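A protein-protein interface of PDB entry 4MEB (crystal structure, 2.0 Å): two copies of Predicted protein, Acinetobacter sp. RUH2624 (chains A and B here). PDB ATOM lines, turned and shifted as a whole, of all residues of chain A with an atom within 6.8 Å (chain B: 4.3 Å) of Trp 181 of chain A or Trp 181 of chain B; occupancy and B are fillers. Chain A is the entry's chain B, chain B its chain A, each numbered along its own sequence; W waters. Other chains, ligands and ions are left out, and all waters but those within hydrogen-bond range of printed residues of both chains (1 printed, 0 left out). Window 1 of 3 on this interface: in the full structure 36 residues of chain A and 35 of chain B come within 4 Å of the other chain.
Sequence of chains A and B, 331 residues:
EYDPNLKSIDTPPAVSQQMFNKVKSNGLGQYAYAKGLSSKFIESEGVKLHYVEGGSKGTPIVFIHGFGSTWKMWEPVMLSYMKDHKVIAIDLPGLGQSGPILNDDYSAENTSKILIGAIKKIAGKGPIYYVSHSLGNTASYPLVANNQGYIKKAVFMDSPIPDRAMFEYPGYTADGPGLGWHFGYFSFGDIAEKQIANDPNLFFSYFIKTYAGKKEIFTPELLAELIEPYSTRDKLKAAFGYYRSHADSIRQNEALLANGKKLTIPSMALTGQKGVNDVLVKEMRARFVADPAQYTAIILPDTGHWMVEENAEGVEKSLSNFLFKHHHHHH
The backbone carbonyl oxygen of Gly 171 of chain A lies close to the backbone NH of Gly 184 of chain B. The backbone NH (N) of Gly 171 of chain B lies within hydrogen-bond range of the backbone carbonyl oxygen (O) of Tyr 169 of chain A.
N of Gly 178 of chain A sits at hydrogen-bond distance from O of Gly 171 of chain A (2.9 Å). O of Pro 170 of chain B lies within hydrogen-bond range of N of Gly 180 of chain B (2.9 Å). OH of Tyr 211 of chain A sits at hydrogen-bond distance from NE1 of Trp 181 of chain A (3.5 Å). O of Pro 170 of chain A sits at hydrogen-bond distance from N of Gly 180 of chain A (2.9 Å). The backbone NH (N) of Gly 178 of chain B lies within hydrogen-bond range of the backbone carbonyl oxygen (O) of Gly 171 of chain B (2.8 Å).
Among the printed residues, pairs that only touch across the chains: Tyr 169 of chain A with Pro 170 of chain B (3.4 Å), Gly 171 of chain A with Gly 171 of chain B (3.8 Å), Gly 171 of chain A with Gly 180 of chain B (3.2 Å), Tyr 172 of chain A with Phe 183 of chain B (3.5 Å), Pro 177 of chain A with Gly 184 of chain B (3.3 Å), Pro 177 of chain A with Phe 188 of chain B (3.7 Å), Gly 180 of chain A with Gly 171 of chain B (3.3 Å), Trp 181 of chain A with Trp 181 of chain B (3.6 Å), Trp 181 of chain A with Gly 184 of chain B (3.7 Å), Trp 181 of chain A with Tyr 185 of chain B (3.6 Å), Trp 181 of chain A with Phe 188 of chain B (3.5 Å), Gly 184 of chain A with Gly 171 of chain B (3.3 Å), Gly 184 of chain A with Pro 177 of chain B (3.5 Å), Gly 184 of chain A with Trp 181 of chain B (3.7 Å), Tyr 185 of chain A with Trp 181 of chain B (3.6 Å), Tyr 185 of chain A with Tyr 185 of chain B (3.7 Å), Phe 188 of chain A with Pro 177 of chain B (3.7 Å), Phe 188 of chain A with Trp 181 of chain B (3.7 Å), Phe 207 of chain A with Phe 188 of chain B (3.9 Å) and Tyr 211 of chain A with Phe 188 of chain B (3.4 Å).
Of the printed residues of chain B, Pro 177 of chain A touches Gly 184 and Phe 188. Trp 181 of chain A touches four residues of chain B. His 182 of chain A touches none of the printed residues of chain B. Of the printed residues of chain B, Tyr 211 of chain A touches Phe 188 (3.4 Å). Of the printed residues of chain A, Pro 177 of chain B touches Gly 184 (3.5 Å) and Phe 188 (3.7 Å). Of chain A, only Trp 181, Gly 184, Tyr 185 and Phe 188 come within 4 Å of Trp 181 of chain B. The nearest printed residue of chain B that does not touch Trp 181 of chain A is Gly 171 of chain B (4.5 Å). The nearest printed residue of chain B that does not touch Gly 171 of chain A is Pro 170 of chain B (4.2 Å).
Printed residues of chain B that touch a printed residue of chain A: Pro 170, Gly 171, Pro 177, Gly 180, Trp 181, Phe 183, Gly 184, Tyr 185 and Phe 188. Of the 21 printed residues of chain A, 11 touch a printed residue of chain B. Printed residues of chain A that touch a printed residue of chain B: Tyr 169, Gly 171, Tyr 172, Pro 177, Gly 180, Trp 181, Gly 184, Tyr 185, Phe 188, Phe 207 and Tyr 211. Hydrophobic or aromatic side chains of chain A that line the printed part of chain B: Tyr 172, Pro 177, Trp 181, Tyr 185, Phe 188, Phe 207 and Tyr 211. Among the printed residues, 22 pairs touch across the chains.
Pro 177 of chain A touches Gly 184 of chain B, and with the chains exchanged Gly 184 of chain A touches Pro 177 of chain B. Pro 177 of chain A touches Phe 188 of chain B, and with the chains exchanged Phe 188 of chain A touches Pro 177 of chain B. Trp 181 of chain A touches Gly 184 of chain B, and with the chains exchanged Gly 184 of chain A touches Trp 181 of chain B. Trp 181 of chain A touches Phe 188 of chain B, and with the chains exchanged Phe 188 of chain A touches Trp 181 of chain B. Of the 22 pairs that touch across the chains among the printed residues, 17 have their exchanged pair printed and touching as well.
Water W1 lies within hydrogen-bond range of O of Tyr 169 of chain A (2.7 Å) and N of Gly 171 of chain B (3.0 Å).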
ATOM      1  N   TYR A   2       7.081 -21.602   6.910  1.00  0.00           N
ATOM      2  CA  TYR A   2       7.868 -22.825   7.099  1.00  0.00           C
ATOM      3  C   TYR A   2       9.058 -22.902   6.141  1.00  0.00           C
ATOM      4  O   TYR A   2       8.895 -22.819   4.924  1.00  0.00           O
ATOM      5  CB  TYR A   2       7.016 -24.099   6.967  1.00  0.00           C
ATOM      6  CG  TYR A   2       7.826 -25.335   7.291  1.00  0.00           C
ATOM      7  CD1 TYR A   2       8.026 -25.726   8.610  1.00  0.00           C
ATOM      8  CD2 TYR A   2       8.434 -26.082   6.287  1.00  0.00           C
ATOM      9  CE1 TYR A   2       8.788 -26.832   8.921  1.00  0.00           C
ATOM     10  CE2 TYR A   2       9.197 -27.196   6.590  1.00  0.00           C
ATOM     11  CZ  TYR A   2       9.372 -27.568   7.909  1.00  0.00           C
ATOM     12  OH  TYR A   2      10.141 -28.667   8.224  1.00  0.00           O
ATOM     13  N   TYR A 169      -8.663 -24.762  10.945  1.00  0.00           N
ATOM     14  CA  TYR A 169      -7.277 -24.555  10.490  1.00  0.00           C
ATOM     15  C   TYR A 169      -6.549 -25.899  10.353  1.00  0.00           C
ATOM     16  O   TYR A 169      -6.530 -26.688  11.286  1.00  0.00           O
ATOM     17  CB  TYR A 169      -6.507 -23.616  11.421  1.00  0.00           C
ATOM     18  CG  TYR A 169      -7.170 -22.264  11.619  1.00  0.00           C
ATOM     19  CD1 TYR A 169      -7.664 -21.537  10.534  1.00  0.00           C
ATOM     20  CD2 TYR A 169      -7.297 -21.718  12.888  1.00  0.00           C
ATOM     21  CE1 TYR A 169      -8.282 -20.298  10.715  1.00  0.00           C
ATOM     22  CE2 TYR A 169      -7.908 -20.479  13.087  1.00  0.00           C
ATOM     23  CZ  TYR A 169      -8.396 -19.774  12.001  1.00  0.00           C
ATOM     24  OH  TYR A 169      -8.999 -18.547  12.214  1.00  0.00           O
ATOM     25  N   PRO A 170      -5.982 -26.167   9.167  1.00  0.00           N
ATOM     26  CA  PRO A 170      -5.388 -27.471   8.864  1.00  0.00           C
ATOM     27  C   PRO A 170      -4.076 -27.722   9.586  1.00  0.00           C
ATOM     28  O   PRO A 170      -3.285 -26.801   9.785  1.00  0.00           O
ATOM     29  CB  PRO A 170      -5.161 -27.407   7.347  1.00  0.00           C
ATOM     30  CG  PRO A 170      -4.995 -25.953   7.063  1.00  0.00           C
ATOM     31  CD  PRO A 170      -5.924 -25.250   8.016  1.00  0.00           C
ATOM     32  N   GLY A 171      -3.844 -28.973   9.977  1.00  0.00           N
ATOM     33  CA  GLY A 171      -2.594 -29.339  10.607  1.00  0.00           C
ATOM     34  C   GLY A 171      -1.451 -29.363   9.605  1.00  0.00           C
ATOM     35  O   GLY A 171      -0.291 -29.161   9.975  1.00  0.00           O
ATOM     36  N   TYR A 172      -1.780 -29.592   8.338  1.00  0.00           N
ATOM     37  CA  TYR A 172      -0.758 -29.777   7.312  1.00  0.00           C
ATOM     38  C   TYR A 172      -1.161 -29.133   5.986  1.00  0.00           C
ATOM     39  O   TYR A 172      -2.351 -29.094   5.635  1.00  0.00           O
ATOM     40  CB  TYR A 172      -0.481 -31.274   7.114  1.00  0.00           C
ATOM     41  CG  TYR A 172       0.712 -31.609   6.246  1.00  0.00           C
ATOM     42  CD1 TYR A 172       2.014 -31.365   6.684  1.00  0.00           C
ATOM     43  CD2 TYR A 172       0.539 -32.197   4.994  1.00  0.00           C
ATOM     44  CE1 TYR A 172       3.112 -31.686   5.895  1.00  0.00           C
ATOM     45  CE2 TYR A 172       1.626 -32.524   4.195  1.00  0.00           C
ATOM     46  CZ  TYR A 172       2.917 -32.267   4.655  1.00  0.00           C
ATOM     47  OH  TYR A 172       4.005 -32.590   3.869  1.00  0.00           O
ATOM     48  N   GLY A 176       3.949 -27.485   4.110  1.00  0.00           N
ATOM     49  CA  GLY A 176       4.375 -28.107   5.359  1.00  0.00           C
ATOM     50  C   GLY A 176       3.405 -27.828   6.497  1.00  0.00           C
ATOM     51  O   GLY A 176       2.238 -27.530   6.240  1.00  0.00           O
ATOM     52  N   PRO A 177       3.879 -27.917   7.755  1.00  0.00           N
ATOM     53  CA  PRO A 177       3.011 -27.744   8.934  1.00  0.00           C
ATOM     54  C   PRO A 177       2.131 -26.498   8.819  1.00  0.00           C
ATOM     55  O   PRO A 177       2.605 -25.442   8.423  1.00  0.00           O
ATOM     56  CB  PRO A 177       4.012 -27.616  10.079  1.00  0.00           C
ATOM     57  CG  PRO A 177       5.148 -28.490   9.639  1.00  0.00           C
ATOM     58  CD  PRO A 177       5.278 -28.172   8.152  1.00  0.00           C
ATOM     59  N   GLY A 178       0.849 -26.651   9.110  1.00  0.00           N
ATOM     60  CA  GLY A 178      -0.099 -25.570   8.946  1.00  0.00           C
ATOM     61  C   GLY A 178      -0.457 -24.866  10.238  1.00  0.00           C
ATOM     62  O   GLY A 178      -0.080 -25.298  11.338  1.00  0.00           O
ATOM     63  N   LEU A 179      -1.193 -23.768  10.088  1.00  0.00           N
ATOM     64  CA  LEU A 179      -1.639 -22.946  11.206  1.00  0.00           C
ATOM     65  C   LEU A 179      -2.323 -23.761  12.309  1.00  0.00           C
ATOM     66  O   LEU A 179      -2.277 -23.402  13.490  1.00  0.00           O
ATOM     67  CB  LEU A 179      -2.601 -21.872  10.684  1.00  0.00           C
ATOM     68  CG  LEU A 179      -3.268 -20.938  11.695  1.00  0.00           C
ATOM     69  CD1 LEU A 179      -2.233 -20.081  12.433  1.00  0.00           C
ATOM     70  CD2 LEU A 179      -4.276 -20.067  10.965  1.00  0.00           C
ATOM     71  N   GLY A 180      -2.968 -24.850  11.917  1.00  0.00           N
ATOM     72  CA  GLY A 180      -3.735 -25.635  12.859  1.00  0.00           C
ATOM     73  C   GLY A 180      -2.935 -26.525  13.792  1.00  0.00           C
ATOM     74  O   GLY A 180      -3.431 -26.888  14.858  1.00  0.00           O
ATOM     75  N   TRP A 181      -1.713 -26.893  13.410  1.00  0.00           N
ATOM     76  CA  TRP A 181      -1.043 -27.985  14.111  1.00  0.00           C
ATOM     77  C   TRP A 181      -0.698 -27.664  15.558  1.00  0.00           C
ATOM     78  O   TRP A 181      -0.841 -28.523  16.427  1.00  0.00           O
ATOM     79  CB  TRP A 181       0.173 -28.534  13.339  1.00  0.00           C
ATOM     80  CG  TRP A 181       1.465 -27.819  13.577  1.00  0.00           C
ATOM     81  CD1 TRP A 181       2.038 -26.867  12.775  1.00  0.00           C
ATOM     82  CD2 TRP A 181       2.373 -28.022  14.669  1.00  0.00           C
ATOM     83  NE1 TRP A 181       3.233 -26.454  13.313  1.00  0.00           N
ATOM     84  CE2 TRP A 181       3.461 -27.141  14.475  1.00  0.00           C
ATOM     85  CE3 TRP A 181       2.365 -28.849  15.800  1.00  0.00           C
ATOM     86  CZ2 TRP A 181       4.533 -27.073  15.362  1.00  0.00           C
ATOM     87  CZ3 TRP A 181       3.430 -28.774  16.683  1.00  0.00           C
ATOM     88  CH2 TRP A 181       4.502 -27.896  16.457  1.00  0.00           C
ATOM     89  N   HIS A 182      -0.280 -26.432  15.834  1.00  0.00           N
ATOM     90  CA  HIS A 182       0.101 -26.103  17.207  1.00  0.00           C
ATOM     91  C   HIS A 182      -1.105 -26.030  18.162  1.00  0.00           C
ATOM     92  O   HIS A 182      -0.967 -26.336  19.335  1.00  0.00           O
ATOM     93  CB  HIS A 182       0.992 -24.851  17.276  1.00  0.00           C
ATOM     94  CG  HIS A 182       0.241 -23.559  17.208  1.00  0.00           C
ATOM     95  ND1 HIS A 182      -0.310 -23.078  16.039  1.00  0.00           N
ATOM     96  CD2 HIS A 182      -0.043 -22.641  18.162  1.00  0.00           C
ATOM     97  CE1 HIS A 182      -0.902 -21.922  16.276  1.00  0.00           C
ATOM     98  NE2 HIS A 182      -0.753 -21.631  17.558  1.00  0.00           N
ATOM     99  N   PHE A 183      -2.281 -25.657  17.654  1.00  0.00           N
ATOM    100  CA  PHE A 183      -3.503 -25.679  18.458  1.00  0.00           C
ATOM    101  C   PHE A 183      -3.771 -27.091  18.992  1.00  0.00           C
ATOM    102  O   PHE A 183      -4.266 -27.263  20.102  1.00  0.00           O
ATOM    103  CB  PHE A 183      -4.708 -25.177  17.653  1.00  0.00           C
ATOM    104  CG  PHE A 183      -4.614 -23.725  17.262  1.00  0.00           C
ATOM    105  CD1 PHE A 183      -4.734 -22.726  18.218  1.00  0.00           C
ATOM    106  CD2 PHE A 183      -4.404 -23.360  15.948  1.00  0.00           C
ATOM    107  CE1 PHE A 183      -4.638 -21.398  17.871  1.00  0.00           C
ATOM    108  CE2 PHE A 183      -4.312 -22.027  15.597  1.00  0.00           C
ATOM    109  CZ  PHE A 183      -4.431 -21.046  16.560  1.00  0.00           C
ATOM    110  N   GLY A 184      -3.430 -28.098  18.196  1.00  0.00           N
ATOM    111  CA  GLY A 184      -3.582 -29.480  18.624  1.00  0.00           C
ATOM    112  C   GLY A 184      -2.467 -29.912  19.566  1.00  0.00           C
ATOM    113  O   GLY A 184      -2.728 -30.425  20.658  1.00  0.00           O
ATOM    114  N   TYR A 185      -1.220 -29.728  19.138  1.00  0.00           N
ATOM    115  CA  TYR A 185      -0.081 -30.175  19.943  1.00  0.00           C
ATOM    116  C   TYR A 185      -0.112 -29.547  21.330  1.00  0.00           C
ATOM    117  O   TYR A 185       0.105 -30.238  22.330  1.00  0.00           O
ATOM    118  CB  TYR A 185       1.250 -29.881  19.243  1.00  0.00           C
ATOM    119  CG  TYR A 185       2.499 -30.219  20.052  1.00  0.00           C
ATOM    120  CD1 TYR A 185       2.721 -31.508  20.537  1.00  0.00           C
ATOM    121  CD2 TYR A 185       3.476 -29.255  20.289  1.00  0.00           C
ATOM    122  CE1 TYR A 185       3.883 -31.818  21.256  1.00  0.00           C
ATOM    123  CE2 TYR A 185       4.632 -29.552  21.000  1.00  0.00           C
ATOM    124  CZ  TYR A 185       4.829 -30.829  21.487  1.00  0.00           C
ATOM    125  OH  TYR A 185       5.982 -31.115  22.191  1.00  0.00           O
ATOM    126  N   PHE A 186      -0.426 -28.252  21.390  1.00  0.00           N
ATOM    127  CA  PHE A 186      -0.409 -27.519  22.662  1.00  0.00           C
ATOM    128  C   PHE A 186      -1.565 -27.907  23.602  1.00  0.00           C
ATOM    129  O   PHE A 186      -1.527 -27.592  24.786  1.00  0.00           O
ATOM    130  CB  PHE A 186      -0.394 -25.997  22.441  1.00  0.00           C
ATOM    131  CG  PHE A 186       0.895 -25.466  21.840  1.00  0.00           C
ATOM    132  CD1 PHE A 186       2.031 -26.267  21.750  1.00  0.00           C
ATOM    133  CD2 PHE A 186       0.968 -24.153  21.379  1.00  0.00           C
ATOM    134  CE1 PHE A 186       3.221 -25.769  21.212  1.00  0.00           C
ATOM    135  CE2 PHE A 186       2.147 -23.645  20.825  1.00  0.00           C
ATOM    136  CZ  PHE A 186       3.275 -24.449  20.743  1.00  0.00           C
ATOM    137  N   PHE A 188      -2.740 -31.203  23.695  1.00  0.00           N
ATOM    138  CA  PHE A 188      -2.662 -32.668  23.716  1.00  0.00           C
ATOM    139  C   PHE A 188      -2.116 -33.114  25.057  1.00  0.00           C
ATOM    140  O   PHE A 188      -0.905 -33.268  25.208  1.00  0.00           O
ATOM    141  CB  PHE A 188      -1.713 -33.101  22.600  1.00  0.00           C
ATOM    142  CG  PHE A 188      -1.649 -34.587  22.351  1.00  0.00           C
ATOM    143  CD1 PHE A 188      -2.746 -35.278  21.862  1.00  0.00           C
ATOM    144  CD2 PHE A 188      -0.448 -35.272  22.513  1.00  0.00           C
ATOM    145  CE1 PHE A 188      -2.667 -36.647  21.584  1.00  0.00           C
ATOM    146  CE2 PHE A 188      -0.350 -36.622  22.233  1.00  0.00           C
ATOM    147  CZ  PHE A 188      -1.468 -37.316  21.763  1.00  0.00           C
ATOM    148  N   ILE A 191       1.696 -33.235  27.222  1.00  0.00           N
ATOM    149  CA  ILE A 191       2.834 -33.677  26.411  1.00  0.00           C
ATOM    150  C   ILE A 191       3.741 -32.519  25.951  1.00  0.00           C
ATOM    151  O   ILE A 191       4.960 -32.620  26.042  1.00  0.00           O
ATOM    152  CB  ILE A 191       2.365 -34.558  25.215  1.00  0.00           C
ATOM    153  CG1 ILE A 191       1.599 -35.794  25.725  1.00  0.00           C
ATOM    154  CG2 ILE A 191       3.535 -34.973  24.339  1.00  0.00           C
ATOM    155  CD1 ILE A 191       2.394 -36.684  26.684  1.00  0.00           C
ATOM    156  N   PHE A 203      13.130 -26.224  21.236  1.00  0.00           N
ATOM    157  CA  PHE A 203      11.815 -26.037  20.633  1.00  0.00           C
ATOM    158  C   PHE A 203      11.590 -24.589  20.203  1.00  0.00           C
ATOM    159  O   PHE A 203      11.211 -24.316  19.063  1.00  0.00           O
ATOM    160  CB  PHE A 203      10.685 -26.484  21.566  1.00  0.00           C
ATOM    161  CG  PHE A 203       9.311 -26.244  20.989  1.00  0.00           C
ATOM    162  CD1 PHE A 203       8.716 -27.194  20.178  1.00  0.00           C
ATOM    163  CD2 PHE A 203       8.632 -25.050  21.222  1.00  0.00           C
ATOM    164  CE1 PHE A 203       7.461 -26.976  19.622  1.00  0.00           C
ATOM    165  CE2 PHE A 203       7.367 -24.829  20.661  1.00  0.00           C
ATOM    166  CZ  PHE A 203       6.789 -25.795  19.865  1.00  0.00           C
ATOM    167  N   PHE A 207      10.920 -22.848  16.708  1.00  0.00           N
ATOM    168  CA  PHE A 207       9.587 -22.278  16.602  1.00  0.00           C
ATOM    169  C   PHE A 207       9.634 -20.771  16.283  1.00  0.00           C
ATOM    170  O   PHE A 207       8.971 -20.306  15.355  1.00  0.00           O
ATOM    171  CB  PHE A 207       8.802 -22.554  17.900  1.00  0.00           C
ATOM    172  CG  PHE A 207       7.381 -22.079  17.870  1.00  0.00           C
ATOM    173  CD1 PHE A 207       6.358 -22.939  17.498  1.00  0.00           C
ATOM    174  CD2 PHE A 207       7.059 -20.781  18.231  1.00  0.00           C
ATOM    175  CE1 PHE A 207       5.040 -22.506  17.480  1.00  0.00           C
ATOM    176  CE2 PHE A 207       5.742 -20.342  18.207  1.00  0.00           C
ATOM    177  CZ  PHE A 207       4.736 -21.205  17.831  1.00  0.00           C
ATOM    178  N   TYR A 211       8.597 -18.770  12.394  1.00  0.00           N
ATOM    179  CA  TYR A 211       7.548 -17.802  12.120  1.00  0.00           C
ATOM    180  C   TYR A 211       8.079 -16.386  11.933  1.00  0.00           C
ATOM    181  O   TYR A 211       7.305 -15.456  11.670  1.00  0.00           O
ATOM    182  CB  TYR A 211       6.436 -17.908  13.167  1.00  0.00           C
ATOM    183  CG  TYR A 211       5.936 -19.332  13.248  1.00  0.00           C
ATOM    184  CD1 TYR A 211       5.232 -19.901  12.193  1.00  0.00           C
ATOM    185  CD2 TYR A 211       6.212 -20.125  14.348  1.00  0.00           C
ATOM    186  CE1 TYR A 211       4.794 -21.220  12.250  1.00  0.00           C
ATOM    187  CE2 TYR A 211       5.782 -21.440  14.415  1.00  0.00           C
ATOM    188  CZ  TYR A 211       5.073 -21.979  13.369  1.00  0.00           C
ATOM    189  OH  TYR A 211       4.642 -23.283  13.444  1.00  0.00           O
ATOM    190  N   PRO B 170      -8.280 -30.750  10.315  1.00  0.00           N
ATOM    191  CA  PRO B 170      -8.053 -29.697  11.316  1.00  0.00           C
ATOM    192  C   PRO B 170      -7.097 -30.111  12.436  1.00  0.00           C
ATOM    193  O   PRO B 170      -7.093 -31.259  12.870  1.00  0.00           O
ATOM    194  CB  PRO B 170      -9.448 -29.466  11.904  1.00  0.00           C
ATOM    195  CG  PRO B 170     -10.396 -30.021  10.884  1.00  0.00           C
ATOM    196  CD  PRO B 170      -9.687 -31.180  10.272  1.00  0.00           C
ATOM    197  N   GLY B 171      -6.287 -29.171  12.899  1.00  0.00           N
ATOM    198  CA  GLY B 171      -5.391 -29.436  14.006  1.00  0.00           C
ATOM    199  C   GLY B 171      -6.156 -29.491  15.318  1.00  0.00           C
ATOM    200  O   GLY B 171      -5.756 -30.200  16.241  1.00  0.00           O
ATOM    201  N   PRO B 177      -7.659 -31.908  20.403  1.00  0.00           N
ATOM    202  CA  PRO B 177      -6.723 -32.128  19.293  1.00  0.00           C
ATOM    203  C   PRO B 177      -7.344 -32.971  18.189  1.00  0.00           C
ATOM    204  O   PRO B 177      -7.979 -33.983  18.479  1.00  0.00           O
ATOM    205  CB  PRO B 177      -5.579 -32.888  19.955  1.00  0.00           C
ATOM    206  CG  PRO B 177      -5.548 -32.334  21.357  1.00  0.00           C
ATOM    207  CD  PRO B 177      -6.986 -31.984  21.713  1.00  0.00           C
ATOM    208  N   GLY B 178      -7.158 -32.551  16.944  1.00  0.00           N
ATOM    209  CA  GLY B 178      -7.816 -33.190  15.821  1.00  0.00           C
ATOM    210  C   GLY B 178      -6.900 -34.069  14.992  1.00  0.00           C
ATOM    211  O   GLY B 178      -5.688 -34.115  15.206  1.00  0.00           O
ATOM    212  N   LEU B 179      -7.497 -34.760  14.030  1.00  0.00           N
ATOM    213  CA  LEU B 179      -6.770 -35.635  13.122  1.00  0.00           C
ATOM    214  C   LEU B 179      -5.571 -34.954  12.480  1.00  0.00           C
ATOM    215  O   LEU B 179      -4.548 -35.588  12.241  1.00  0.00           O
ATOM    216  CB  LEU B 179      -7.720 -36.131  12.026  1.00  0.00           C
ATOM    217  CG  LEU B 179      -7.112 -36.987  10.904  1.00  0.00           C
ATOM    218  CD1 LEU B 179      -6.448 -38.231  11.484  1.00  0.00           C
ATOM    219  CD2 LEU B 179      -8.210 -37.374   9.914  1.00  0.00           C
ATOM    220  N   GLY B 180      -5.687 -33.661  12.207  1.00  0.00           N
ATOM    221  CA  GLY B 180      -4.639 -32.971  11.479  1.00  0.00           C
ATOM    222  C   GLY B 180      -3.375 -32.601  12.245  1.00  0.00           C
ATOM    223  O   GLY B 180      -2.323 -32.404  11.624  1.00  0.00           O
ATOM    224  N   TRP B 181      -3.450 -32.487  13.570  1.00  0.00           N
ATOM    225  CA  TRP B 181      -2.326 -31.894  14.300  1.00  0.00           C
ATOM    226  C   TRP B 181      -1.024 -32.683  14.148  1.00  0.00           C
ATOM    227  O   TRP B 181       0.031 -32.079  13.943  1.00  0.00           O
ATOM    228  CB  TRP B 181      -2.650 -31.599  15.781  1.00  0.00           C
ATOM    229  CG  TRP B 181      -2.483 -32.771  16.722  1.00  0.00           C
ATOM    230  CD1 TRP B 181      -3.460 -33.604  17.164  1.00  0.00           C
ATOM    231  CD2 TRP B 181      -1.262 -33.226  17.332  1.00  0.00           C
ATOM    232  NE1 TRP B 181      -2.932 -34.556  18.012  1.00  0.00           N
ATOM    233  CE2 TRP B 181      -1.583 -34.346  18.128  1.00  0.00           C
ATOM    234  CE3 TRP B 181       0.071 -32.797  17.281  1.00  0.00           C
ATOM    235  CZ2 TRP B 181      -0.628 -35.042  18.861  1.00  0.00           C
ATOM    236  CZ3 TRP B 181       1.015 -33.482  18.015  1.00  0.00           C
ATOM    237  CH2 TRP B 181       0.661 -34.597  18.796  1.00  0.00           C
ATOM    238  N   HIS B 182      -1.088 -34.012  14.193  1.00  0.00           N
ATOM    239  CA  HIS B 182       0.144 -34.793  14.146  1.00  0.00           C
ATOM    240  C   HIS B 182       0.837 -34.737  12.775  1.00  0.00           C
ATOM    241  O   HIS B 182       2.050 -34.926  12.685  1.00  0.00           O
ATOM    242  CB  HIS B 182      -0.072 -36.237  14.624  1.00  0.00           C
ATOM    243  CG  HIS B 182      -0.690 -37.138  13.599  1.00  0.00           C
ATOM    244  ND1 HIS B 182      -2.022 -37.066  13.250  1.00  0.00           N
ATOM    245  CD2 HIS B 182      -0.165 -38.148  12.866  1.00  0.00           C
ATOM    246  CE1 HIS B 182      -2.286 -37.977  12.331  1.00  0.00           C
ATOM    247  NE2 HIS B 182      -1.179 -38.653  12.085  1.00  0.00           N
ATOM    248  N   PHE B 183       0.072 -34.466  11.717  1.00  0.00           N
ATOM    249  CA  PHE B 183       0.647 -34.322  10.380  1.00  0.00           C
ATOM    250  C   PHE B 183       1.579 -33.109  10.341  1.00  0.00           C
ATOM    251  O   PHE B 183       2.591 -33.110   9.632  1.00  0.00           O
ATOM    252  CB  PHE B 183      -0.448 -34.195   9.310  1.00  0.00           C
ATOM    253  CG  PHE B 183      -1.245 -35.461   9.091  1.00  0.00           C
ATOM    254  CD1 PHE B 183      -0.670 -36.565   8.487  1.00  0.00           C
ATOM    255  CD2 PHE B 183      -2.581 -35.536   9.476  1.00  0.00           C
ATOM    256  CE1 PHE B 183      -1.407 -37.736   8.278  1.00  0.00           C
ATOM    257  CE2 PHE B 183      -3.325 -36.695   9.261  1.00  0.00           C
ATOM    258  CZ  PHE B 183      -2.731 -37.800   8.665  1.00  0.00           C
ATOM    259  N   GLY B 184       1.225 -32.083  11.107  1.00  0.00           N
ATOM    260  CA  GLY B 184       2.034 -30.891  11.231  1.00  0.00           C
ATOM    261  C   GLY B 184       3.200 -31.075  12.187  1.00  0.00           C
ATOM    262  O   GLY B 184       4.344 -30.738  11.852  1.00  0.00           O
ATOM    263  N   TYR B 185       2.922 -31.605  13.380  1.00  0.00           N
ATOM    264  CA  TYR B 185       3.987 -31.807  14.374  1.00  0.00           C
ATOM    265  C   TYR B 185       5.100 -32.693  13.829  1.00  0.00           C
ATOM    266  O   TYR B 185       6.283 -32.382  13.982  1.00  0.00           O
ATOM    267  CB  TYR B 185       3.423 -32.409  15.664  1.00  0.00           C
ATOM    268  CG  TYR B 185       4.458 -32.732  16.741  1.00  0.00           C
ATOM    269  CD1 TYR B 185       5.410 -31.793  17.135  1.00  0.00           C
ATOM    270  CD2 TYR B 185       4.451 -33.967  17.385  1.00  0.00           C
ATOM    271  CE1 TYR B 185       6.343 -32.090  18.136  1.00  0.00           C
ATOM    272  CE2 TYR B 185       5.376 -34.275  18.377  1.00  0.00           C
ATOM    273  CZ  TYR B 185       6.320 -33.335  18.751  1.00  0.00           C
ATOM    274  OH  TYR B 185       7.237 -33.647  19.741  1.00  0.00           O
ATOM    275  N   PHE B 188       7.467 -30.899  11.323  1.00  0.00           N
ATOM    276  CA  PHE B 188       7.994 -29.632  11.826  1.00  0.00           C
ATOM    277  C   PHE B 188       9.486 -29.794  12.130  1.00  0.00           C
ATOM    278  O   PHE B 188       9.857 -30.139  13.250  1.00  0.00           O
ATOM    279  CB  PHE B 188       7.215 -29.284  13.095  1.00  0.00           C
ATOM    280  CG  PHE B 188       7.469 -27.903  13.652  1.00  0.00           C
ATOM    281  CD1 PHE B 188       7.078 -26.770  12.963  1.00  0.00           C
ATOM    282  CD2 PHE B 188       8.005 -27.751  14.926  1.00  0.00           C
ATOM    283  CE1 PHE B 188       7.263 -25.504  13.506  1.00  0.00           C
ATOM    284  CE2 PHE B 188       8.191 -26.492  15.477  1.00  0.00           C
ATOM    285  CZ  PHE B 188       7.819 -25.366  14.759  1.00  0.00           C
HETATM  286  O   HOH W   1      -7.542 -26.581  13.740  1.00  0.00           O
